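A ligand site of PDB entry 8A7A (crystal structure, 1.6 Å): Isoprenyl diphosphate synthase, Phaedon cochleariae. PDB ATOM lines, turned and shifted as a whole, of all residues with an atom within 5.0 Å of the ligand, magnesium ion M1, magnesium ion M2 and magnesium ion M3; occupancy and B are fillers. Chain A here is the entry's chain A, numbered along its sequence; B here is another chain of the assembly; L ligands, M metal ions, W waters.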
ATOM      1  N   LEU A  92       5.728 -15.363   5.546  1.00  0.00           N
ATOM      2  CA  LEU A  92       5.528 -16.606   4.752  1.00  0.00           C
ATOM      3  C   LEU A  92       6.181 -16.426   3.371  1.00  0.00           C
ATOM      4  O   LEU A  92       6.836 -17.377   2.902  1.00  0.00           O
ATOM      5  CB  LEU A  92       4.031 -16.915   4.595  1.00  0.00           C
ATOM      6  CG  LEU A  92       3.265 -17.229   5.880  1.00  0.00           C
ATOM      7  CD1 LEU A  92       1.786 -17.342   5.585  1.00  0.00           C
ATOM      8  CD2 LEU A  92       3.783 -18.502   6.540  1.00  0.00           C
ATOM      9  N   LEU A  93       6.034 -15.245   2.771  1.00  0.00           N
ATOM     10  CA  LEU A  93       6.515 -14.991   1.389  1.00  0.00           C
ATOM     11  C   LEU A  93       8.033 -14.772   1.378  1.00  0.00           C
ATOM     12  O   LEU A  93       8.683 -15.240   0.404  1.00  0.00           O
ATOM     13  CB  LEU A  93       5.735 -13.811   0.794  1.00  0.00           C
ATOM     14  CG  LEU A  93       4.222 -14.013   0.719  1.00  0.00           C
ATOM     15  CD1 LEU A  93       3.567 -12.870  -0.037  1.00  0.00           C
ATOM     16  CD2 LEU A  93       3.864 -15.343   0.053  1.00  0.00           C
ATOM     17  N   MET A  95      10.042 -16.404   3.266  1.00  0.00           N
ATOM     18  CA  MET A  95      10.558 -17.798   3.389  1.00  0.00           C
ATOM     19  C   MET A  95      10.321 -18.552   2.079  1.00  0.00           C
ATOM     20  O   MET A  95      11.258 -19.214   1.596  1.00  0.00           O
ATOM     21  CB  MET A  95       9.911 -18.554   4.546  1.00  0.00           C
ATOM     22  CG  MET A  95      10.396 -19.992   4.667  1.00  0.00           C
ATOM     23  SD  MET A  95      10.062 -20.723   6.297  1.00  0.00           S
ATOM     24  CE  MET A  95      11.482 -20.128   7.213  1.00  0.00           C
ATOM     25  N   ASP A  96       9.106 -18.462   1.534  1.00  0.00           N
ATOM     26  CA  ASP A  96       8.719 -19.206   0.298  1.00  0.00           C
ATOM     27  C   ASP A  96       9.685 -18.823  -0.832  1.00  0.00           C
ATOM     28  O   ASP A  96      10.136 -19.731  -1.564  1.00  0.00           O
ATOM     29  CB  ASP A  96       7.272 -18.934  -0.105  1.00  0.00           C
ATOM     30  CG  ASP A  96       6.910 -19.656  -1.388  1.00  0.00           C
ATOM     31  OD1 ASP A  96       6.622 -20.875  -1.308  1.00  0.00           O
ATOM     32  OD2 ASP A  96       6.975 -19.006  -2.459  1.00  0.00           O
ATOM     33  N   ASP A  97       9.987 -17.532  -0.979  1.00  0.00           N
ATOM     34  CA  ASP A  97      10.861 -17.025  -2.066  1.00  0.00           C
ATOM     35  C   ASP A  97      12.268 -17.622  -1.930  1.00  0.00           C
ATOM     36  O   ASP A  97      12.869 -17.942  -2.987  1.00  0.00           O
ATOM     37  CB  ASP A  97      10.859 -15.499  -2.104  1.00  0.00           C
ATOM     38  CG  ASP A  97       9.581 -14.921  -2.675  1.00  0.00           C
ATOM     39  OD1 ASP A  97       8.924 -15.624  -3.480  1.00  0.00           O
ATOM     40  OD2 ASP A  97       9.216 -13.785  -2.297  1.00  0.00           O
ATOM     41  N   MET A  99      12.902 -20.598  -0.479  1.00  0.00           N
ATOM     42  CA  MET A  99      12.678 -22.044  -0.733  1.00  0.00           C
ATOM     43  C   MET A  99      12.559 -22.298  -2.249  1.00  0.00           C
ATOM     44  O   MET A  99      13.134 -23.307  -2.724  1.00  0.00           O
ATOM     45  CB  MET A  99      11.420 -22.549  -0.018  1.00  0.00           C
ATOM     46  CG  MET A  99      11.635 -22.720   1.468  1.00  0.00           C
ATOM     47  SD  MET A  99      10.144 -23.175   2.403  1.00  0.00           S
ATOM     48  CE  MET A  99       9.790 -24.806   1.750  1.00  0.00           C
ATOM     49  N   ASP A 100      11.873 -21.408  -2.973  1.00  0.00           N
ATOM     50  CA  ASP A 100      11.609 -21.574  -4.430  1.00  0.00           C
ATOM     51  C   ASP A 100      12.695 -20.903  -5.274  1.00  0.00           C
ATOM     52  O   ASP A 100      12.679 -21.079  -6.512  1.00  0.00           O
ATOM     53  CB  ASP A 100      10.210 -21.043  -4.778  1.00  0.00           C
ATOM     54  CG  ASP A 100       9.110 -21.843  -4.109  1.00  0.00           C
ATOM     55  OD1 ASP A 100       9.373 -23.004  -3.728  1.00  0.00           O
ATOM     56  OD2 ASP A 100       8.000 -21.291  -3.964  1.00  0.00           O
ATOM     57  N   SER A 102      13.084 -17.826  -6.060  1.00  0.00           N
ATOM     58  CA  SER A 102      12.421 -16.881  -7.003  1.00  0.00           C
ATOM     59  C   SER A 102      13.258 -15.611  -7.150  1.00  0.00           C
ATOM     60  O   SER A 102      13.995 -15.260  -6.209  1.00  0.00           O
ATOM     61  CB  SER A 102      11.016 -16.581  -6.554  1.00  0.00           C
ATOM     62  OG  SER A 102      10.224 -17.756  -6.581  1.00  0.00           O
ATOM     63  N   ARG A 105       9.020 -10.852  -6.444  1.00  0.00           N
ATOM     64  CA  ARG A 105       7.593 -10.964  -6.048  1.00  0.00           C
ATOM     65  C   ARG A 105       6.925  -9.601  -6.266  1.00  0.00           C
ATOM     66  O   ARG A 105       7.396  -8.617  -5.663  1.00  0.00           O
ATOM     67  CB  ARG A 105       7.440 -11.408  -4.596  1.00  0.00           C
ATOM     68  CG  ARG A 105       5.989 -11.608  -4.188  1.00  0.00           C
ATOM     69  CD  ARG A 105       5.838 -12.250  -2.842  1.00  0.00           C
ATOM     70  NE  ARG A 105       6.330 -13.626  -2.808  1.00  0.00           N
ATOM     71  CZ  ARG A 105       5.663 -14.690  -3.217  1.00  0.00           C
ATOM     72  NH1 ARG A 105       4.439 -14.585  -3.730  1.00  0.00           N
ATOM     73  NH2 ARG A 105       6.208 -15.895  -3.114  1.00  0.00           N
ATOM     74  N   THR A 160      -0.508 -23.650   8.086  1.00  0.00           N
ATOM     75  CA  THR A 160       0.127 -23.103   6.862  1.00  0.00           C
ATOM     76  C   THR A 160       1.437 -23.869   6.600  1.00  0.00           C
ATOM     77  O   THR A 160       1.720 -24.173   5.417  1.00  0.00           O
ATOM     78  CB  THR A 160       0.328 -21.584   6.934  1.00  0.00           C
ATOM     79  OG1 THR A 160      -0.938 -20.980   7.211  1.00  0.00           O
ATOM     80  CG2 THR A 160       0.883 -21.018   5.648  1.00  0.00           C
ATOM     81  N   ASN A 161       2.182 -24.174   7.661  1.00  0.00           N
ATOM     82  CA  ASN A 161       3.431 -24.969   7.555  1.00  0.00           C
ATOM     83  C   ASN A 161       3.116 -26.373   7.047  1.00  0.00           C
ATOM     84  O   ASN A 161       3.871 -26.881   6.208  1.00  0.00           O
ATOM     85  CB  ASN A 161       4.226 -24.992   8.867  1.00  0.00           C
ATOM     86  CG  ASN A 161       5.165 -23.807   8.957  1.00  0.00           C
ATOM     87  OD1 ASN A 161       6.219 -23.795   8.319  1.00  0.00           O
ATOM     88  ND2 ASN A 161       4.788 -22.803   9.737  1.00  0.00           N
ATOM     89  N   GLN A 164       2.608 -25.975   3.304  1.00  0.00           N
ATOM     90  CA  GLN A 164       3.895 -25.732   2.600  1.00  0.00           C
ATOM     91  C   GLN A 164       4.648 -27.058   2.470  1.00  0.00           C
ATOM     92  O   GLN A 164       5.149 -27.355   1.375  1.00  0.00           O
ATOM     93  CB  GLN A 164       4.728 -24.664   3.320  1.00  0.00           C
ATOM     94  CG  GLN A 164       6.046 -24.323   2.626  1.00  0.00           C
ATOM     95  CD  GLN A 164       5.893 -23.433   1.415  1.00  0.00           C
ATOM     96  OE1 GLN A 164       4.868 -23.407   0.755  1.00  0.00           O
ATOM     97  NE2 GLN A 164       6.951 -22.685   1.106  1.00  0.00           N
ATOM     98  N   ASP A 167       2.962 -29.332  -0.097  1.00  0.00           N
ATOM     99  CA  ASP A 167       3.338 -28.787  -1.431  1.00  0.00           C
ATOM    100  C   ASP A 167       4.726 -29.320  -1.806  1.00  0.00           C
ATOM    101  O   ASP A 167       4.912 -29.720  -2.982  1.00  0.00           O
ATOM    102  CB  ASP A 167       3.282 -27.252  -1.408  1.00  0.00           C
ATOM    103  CG  ASP A 167       3.160 -26.607  -2.782  1.00  0.00           C
ATOM    104  OD1 ASP A 167       2.668 -27.268  -3.719  1.00  0.00           O
ATOM    105  OD2 ASP A 167       3.538 -25.429  -2.896  1.00  0.00           O
ATOM    106  N   LYS A 193      -2.211 -24.484   2.920  1.00  0.00           N
ATOM    107  CA  LYS A 193      -1.125 -23.544   2.539  1.00  0.00           C
ATOM    108  C   LYS A 193      -1.658 -22.111   2.375  1.00  0.00           C
ATOM    109  O   LYS A 193      -0.887 -21.179   2.642  1.00  0.00           O
ATOM    110  CB  LYS A 193      -0.421 -23.974   1.260  1.00  0.00           C
ATOM    111  CG  LYS A 193       0.900 -23.270   0.986  1.00  0.00           C
ATOM    112  CD  LYS A 193       1.506 -23.584  -0.372  1.00  0.00           C
ATOM    113  CE  LYS A 193       0.800 -22.874  -1.509  1.00  0.00           C
ATOM    114  NZ  LYS A 193       1.413 -23.195  -2.819  1.00  0.00           N
ATOM    115  N   THR A 194      -2.905 -21.930   1.915  1.00  0.00           N
ATOM    116  CA  THR A 194      -3.395 -20.597   1.448  1.00  0.00           C
ATOM    117  C   THR A 194      -4.733 -20.216   2.077  1.00  0.00           C
ATOM    118  O   THR A 194      -4.820 -19.088   2.577  1.00  0.00           O
ATOM    119  CB  THR A 194      -3.427 -20.535  -0.091  1.00  0.00           C
ATOM    120  OG1 THR A 194      -4.499 -21.319  -0.610  1.00  0.00           O
ATOM    121  CG2 THR A 194      -2.142 -21.025  -0.702  1.00  0.00           C
ATOM    122  N   TYR A 197      -5.002 -18.920   5.996  1.00  0.00           N
ATOM    123  CA  TYR A 197      -4.440 -17.587   6.347  1.00  0.00           C
ATOM    124  C   TYR A 197      -5.080 -16.491   5.481  1.00  0.00           C
ATOM    125  O   TYR A 197      -5.169 -15.349   5.938  1.00  0.00           O
ATOM    126  CB  TYR A 197      -2.909 -17.587   6.322  1.00  0.00           C
ATOM    127  CG  TYR A 197      -2.281 -17.119   5.025  1.00  0.00           C
ATOM    128  CD1 TYR A 197      -2.044 -15.770   4.802  1.00  0.00           C
ATOM    129  CD2 TYR A 197      -1.891 -18.023   4.062  1.00  0.00           C
ATOM    130  CE1 TYR A 197      -1.468 -15.328   3.620  1.00  0.00           C
ATOM    131  CE2 TYR A 197      -1.316 -17.603   2.872  1.00  0.00           C
ATOM    132  CZ  TYR A 197      -1.093 -16.259   2.650  1.00  0.00           C
ATOM    133  OH  TYR A 197      -0.521 -15.840   1.490  1.00  0.00           O
ATOM    134  N   THR A 253       4.935 -18.417 -14.475  1.00  0.00           N
ATOM    135  CA  THR A 253       6.108 -19.329 -14.471  1.00  0.00           C
ATOM    136  C   THR A 253       5.790 -20.628 -13.715  1.00  0.00           C
ATOM    137  O   THR A 253       6.748 -21.365 -13.409  1.00  0.00           O
ATOM    138  CB  THR A 253       7.337 -18.617 -13.885  1.00  0.00           C
ATOM    139  OG1 THR A 253       7.002 -18.117 -12.592  1.00  0.00           O
ATOM    140  CG2 THR A 253       7.821 -17.474 -14.760  1.00  0.00           C
ATOM    141  N   GLU A 257       8.349 -23.843 -12.991  1.00  0.00           N
ATOM    142  CA  GLU A 257       8.591 -24.072 -11.542  1.00  0.00           C
ATOM    143  C   GLU A 257       8.113 -25.478 -11.126  1.00  0.00           C
ATOM    144  O   GLU A 257       8.465 -25.915 -10.013  1.00  0.00           O
ATOM    145  CB  GLU A 257       7.916 -22.961 -10.737  1.00  0.00           C
ATOM    146  CG  GLU A 257       8.609 -21.609 -10.888  1.00  0.00           C
ATOM    147  CD  GLU A 257       7.857 -20.390 -10.368  1.00  0.00           C
ATOM    148  OE1 GLU A 257       8.521 -19.373 -10.091  1.00  0.00           O
ATOM    149  OE2 GLU A 257       6.617 -20.449 -10.248  1.00  0.00           O
ATOM    150  N   LYS A 259       5.001 -26.542 -10.515  1.00  0.00           N
ATOM    151  CA  LYS A 259       4.002 -26.416  -9.417  1.00  0.00           C
ATOM    152  C   LYS A 259       2.898 -27.464  -9.597  1.00  0.00           C
ATOM    153  O   LYS A 259       2.553 -27.794 -10.741  1.00  0.00           O
ATOM    154  CB  LYS A 259       3.386 -25.024  -9.397  1.00  0.00           C
ATOM    155  CG  LYS A 259       4.324 -23.936  -8.906  1.00  0.00           C
ATOM    156  CD  LYS A 259       3.585 -22.761  -8.331  1.00  0.00           C
ATOM    157  CE  LYS A 259       4.479 -21.575  -8.061  1.00  0.00           C
ATOM    158  NZ  LYS A 259       3.714 -20.310  -8.172  1.00  0.00           N
ATOM    159  N   ASN B 123      11.294 -24.557   6.014  1.00  0.00           N
ATOM    160  CA  ASN B 123      10.112 -24.155   6.816  1.00  0.00           C
ATOM    161  C   ASN B 123       9.958 -25.056   8.045  1.00  0.00           C
ATOM    162  O   ASN B 123       9.104 -24.750   8.905  1.00  0.00           O
ATOM    163  CB  ASN B 123       8.823 -24.111   5.996  1.00  0.00           C
ATOM    164  CG  ASN B 123       8.319 -25.480   5.601  1.00  0.00           C
ATOM    165  OD1 ASN B 123       8.992 -26.195   4.859  1.00  0.00           O
ATOM    166  ND2 ASN B 123       7.136 -25.853   6.062  1.00  0.00           N
ATOM    167  N   LEU B 126      10.435 -22.946  11.243  1.00  0.00           N
ATOM    168  CA  LEU B 126       9.205 -22.170  11.568  1.00  0.00           C
ATOM    169  C   LEU B 126       8.157 -23.119  12.172  1.00  0.00           C
ATOM    170  O   LEU B 126       7.517 -22.741  13.185  1.00  0.00           O
ATOM    171  CB  LEU B 126       8.667 -21.510  10.298  1.00  0.00           C
ATOM    172  CG  LEU B 126       7.447 -20.611  10.476  1.00  0.00           C
ATOM    173  CD1 LEU B 126       7.742 -19.432  11.386  1.00  0.00           C
ATOM    174  CD2 LEU B 126       6.949 -20.117   9.116  1.00  0.00           C
HETATM  175  C1  LIG L   1       2.772 -20.010   1.782  1.00  0.00           C
HETATM  176  C2  LIG L   1       4.223 -20.238   2.153  1.00  0.00           C
HETATM  177  C3  LIG L   1       4.126 -21.060   3.434  1.00  0.00           C
HETATM  178  C4  LIG L   1       5.276 -21.208   4.430  1.00  0.00           C
HETATM  179  C5  LIG L   1       5.036 -22.031   5.699  1.00  0.00           C
HETATM  180  O1  LIG L   1       4.447 -17.895  -7.055  1.00  0.00           O
HETATM  181  P1  LIG L   1       4.294 -18.135  -5.464  1.00  0.00           P
HETATM  182  O2  LIG L   1       3.252 -16.995  -4.955  1.00  0.00           O
HETATM  183  O3  LIG L   1       5.593 -18.063  -4.755  1.00  0.00           O
HETATM  184  O4  LIG L   1       3.538 -19.553  -5.378  1.00  0.00           O
HETATM  185  P2  LIG L   1       3.792 -20.690  -4.259  1.00  0.00           P
HETATM  186  O5  LIG L   1       5.358 -20.824  -3.991  1.00  0.00           O
HETATM  187  O6  LIG L   1       3.202 -21.970  -4.705  1.00  0.00           O
HETATM  188  O7  LIG L   1       3.110 -20.197  -2.899  1.00  0.00           O
HETATM  189  C6  LIG L   1       3.548 -19.105  -2.118  1.00  0.00           C
HETATM  190  C7  LIG L   1       3.676 -19.707  -0.705  1.00  0.00           C
HETATM  191  C8  LIG L   1       2.687 -19.386   0.415  1.00  0.00           C
HETATM  192 BR1  LIG L   1       1.238 -18.257   0.056  1.00  0.00          BR
HETATM  193  C9  LIG L   1       6.647 -20.549   4.209  1.00  0.00           C
HETATM  194 MG    MG M   1       6.402 -22.282  -2.876  1.00  0.00          MG
HETATM  195 MG    MG M   2       5.295 -16.810  -8.416  1.00  0.00          MG
HETATM  196 MG    MG M   3       6.935 -19.502  -4.401  1.00  0.00          MG
HETATM  197  O   HOH W   1       3.942 -24.416  -5.330  1.00  0.00           O
HETATM  198  O   HOH W   2       1.176 -21.410  -6.777  1.00  0.00           O
HETATM  199  O   HOH W   3       7.140 -19.936  -6.432  1.00  0.00           O
HETATM  200  O   HOH W   4       7.668 -23.576  -1.844  1.00  0.00           O
HETATM  201  O   HOH W   5       6.027 -15.544  -9.844  1.00  0.00           O
HETATM  202  O   HOH W   6       6.383 -23.679  -4.361  1.00  0.00           O
HETATM  203  O   HOH W   7       7.187 -17.701  -7.927  1.00  0.00           O
HETATM  204  O   HOH W   8      -0.180 -20.518  -3.746  1.00  0.00           O
HETATM  205  O   HOH W   9      -1.260 -16.860  -1.329  1.00  0.00           O
HETATM  206  O   HOH W  10       3.350 -16.136  -8.903  1.00  0.00           O
HETATM  207  O   HOH W  11       4.734 -23.084  -1.883  1.00  0.00           O
HETATM  208  O   HOH W  12       5.004 -18.307  -9.881  1.00  0.00           O
HETATM  209  O   HOH W  13       2.052 -15.398  -6.654  1.00  0.00           O
HETATM  210  O   HOH W  14       8.459 -18.200  -4.634  1.00  0.00           O
HETATM  211  O   HOH W  15       5.547 -15.231  -7.059  1.00  0.00           O
HETATM  212  O   HOH W  16       0.749 -17.844  -4.480  1.00  0.00           O
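Merely in contact with magnesium ion M2: Lys 259.
Of the 21 residues printed, 1 comes within 4 Å of magnesium ion M2.
The side-chain amino group (NZ) of Lys 259 lies within salt-bridge range of an oxygen (O6) of the ligand (3.9 Å).
An oxygen (O2) of the ligand is in salt-bridge range of the guanidinium group (NH1) of Arg 105 (3.0 Å).
The side-chain amino group (NZ) of Lys 193 is in salt-bridge range of an oxygen (O6) of the ligand.
Two residues have an atom within 4 Å of magnesium ion M1: Asp 96 and Asp 100.
Magnesium ion M2 is bound by O1 of the ligand (1.9 Å), water W5 (2.0 Å), water W15 (2.1 Å), water W12 (2.1 Å), water W10 (2.1 Å) and water W7 (2.1 Å).
Magnesium ion M2 has six donor atoms within binding distance.
Leu 92 touches the ligand.
Leu 93 touches the ligand (CD2 to BR1, 3.9 Å).
Met 95 touches the ligand.
Thr 160 touches the ligand (CG2 to C3, 3.9 Å).
Asn 161 touches the ligand.
Gln 164 touches the ligand (OE1 to C2, 3.5 Å).
Asp 167 touches the ligand.
Tyr 197 touches the ligand.
13 residues have an atom within 4 Å of the ligand: Leu 92, Leu 93, Met 95, Asp 96, Asp 100, Arg 105, Thr 160, Asn 161, Gln 164, Asp 167, Lys 193, Tyr 197 and Lys 259.
Merely in contact with magnesium ion M3: Arg 105 (3.9 Å).
Of the 21 residues printed, 3 come within 4 Å of magnesium ion M3.
The nearest printed residue that does not touch magnesium ion M3 is Ser 102 (4.3 Å).
Water W6 is bound to magnesium ion M1 (2.0 Å).
Water W4 is bound to magnesium ion M1 (2.1 Å).
Water W11 is bound to magnesium ion M1.
O5 of the ligand binds magnesium ion M1, at 2.1 Å.
Magnesium ion M1 is bound by OD1 of Asp 96 (2.1 Å).
The side-chain carboxylate (OD2) of Asp 100 is bound to magnesium ion M1, 2.2 Å away.
Magnesium ion M1 has six donor atoms within binding distance.
The guanidinium group of Arg 105 sits close to the side-chain carboxylate of Asp 96 (3.3 Å).
The side-chain amide nitrogen of Gln 164 sits close to the side-chain carboxylate of Asp 96.
The side-chain amino group (NZ) of Lys 259 lies within salt-bridge range of the side-chain carboxylate (OE2) of Glu 257.
The guanidinium group (NH2) of Arg 105 lies within salt-bridge range of the side-chain carboxylate (OD1) of Asp 97.
OD2 of Asp 167 lies within salt-bridge range of NZ of Lys 193, 3.1 Å away.
O of Asn 123 of chain B sits close to OD1 of Asn 161 (3.1 Å).
NE2 of Gln 164 sits at hydrogen-bond distance from SD of Met 99 (3.5 Å).
Magnesium ion M3 is bound by an oxygen (O3) of the ligand, the side-chain carboxylate of Asp 96, water W14, water W3, an oxygen (O5) of the ligand and the side-chain carboxylate of Asp 100.
Magnesium ion M3 has six donor atoms within binding distance.
Water W11 lies within hydrogen-bond range of OE1 of Gln 164 (2.7 Å), OD2 of Asp 167 (2.8 Å), O6 of the ligand (3.4 Å) and NZ of Lys 193 (3.5 Å).
Water W4 bridges the side-chain carboxylate of Asp 100 (2.6 Å) and the side-chain amide nitrogen of Gln 164 (3.2 Å).
Water W12 lies within hydrogen-bond range of OE2 of Glu 257 (2.7 Å), NZ of Lys 259 (2.9 Å) and OG1 of Thr 253 (3.4 Å).
Water W1 bridges an oxygen (O6) of the ligand (2.6 Å) and the side-chain carboxylate of Asp 167 (2.7 Å).
Water W2 lies within hydrogen-bond range of O6 of the ligand (3.0 Å) and NZ of Lys 259 (3.1 Å).
Water W8 bridges the side-chain amino group of Lys 193 and an oxygen (O7) of the ligand.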
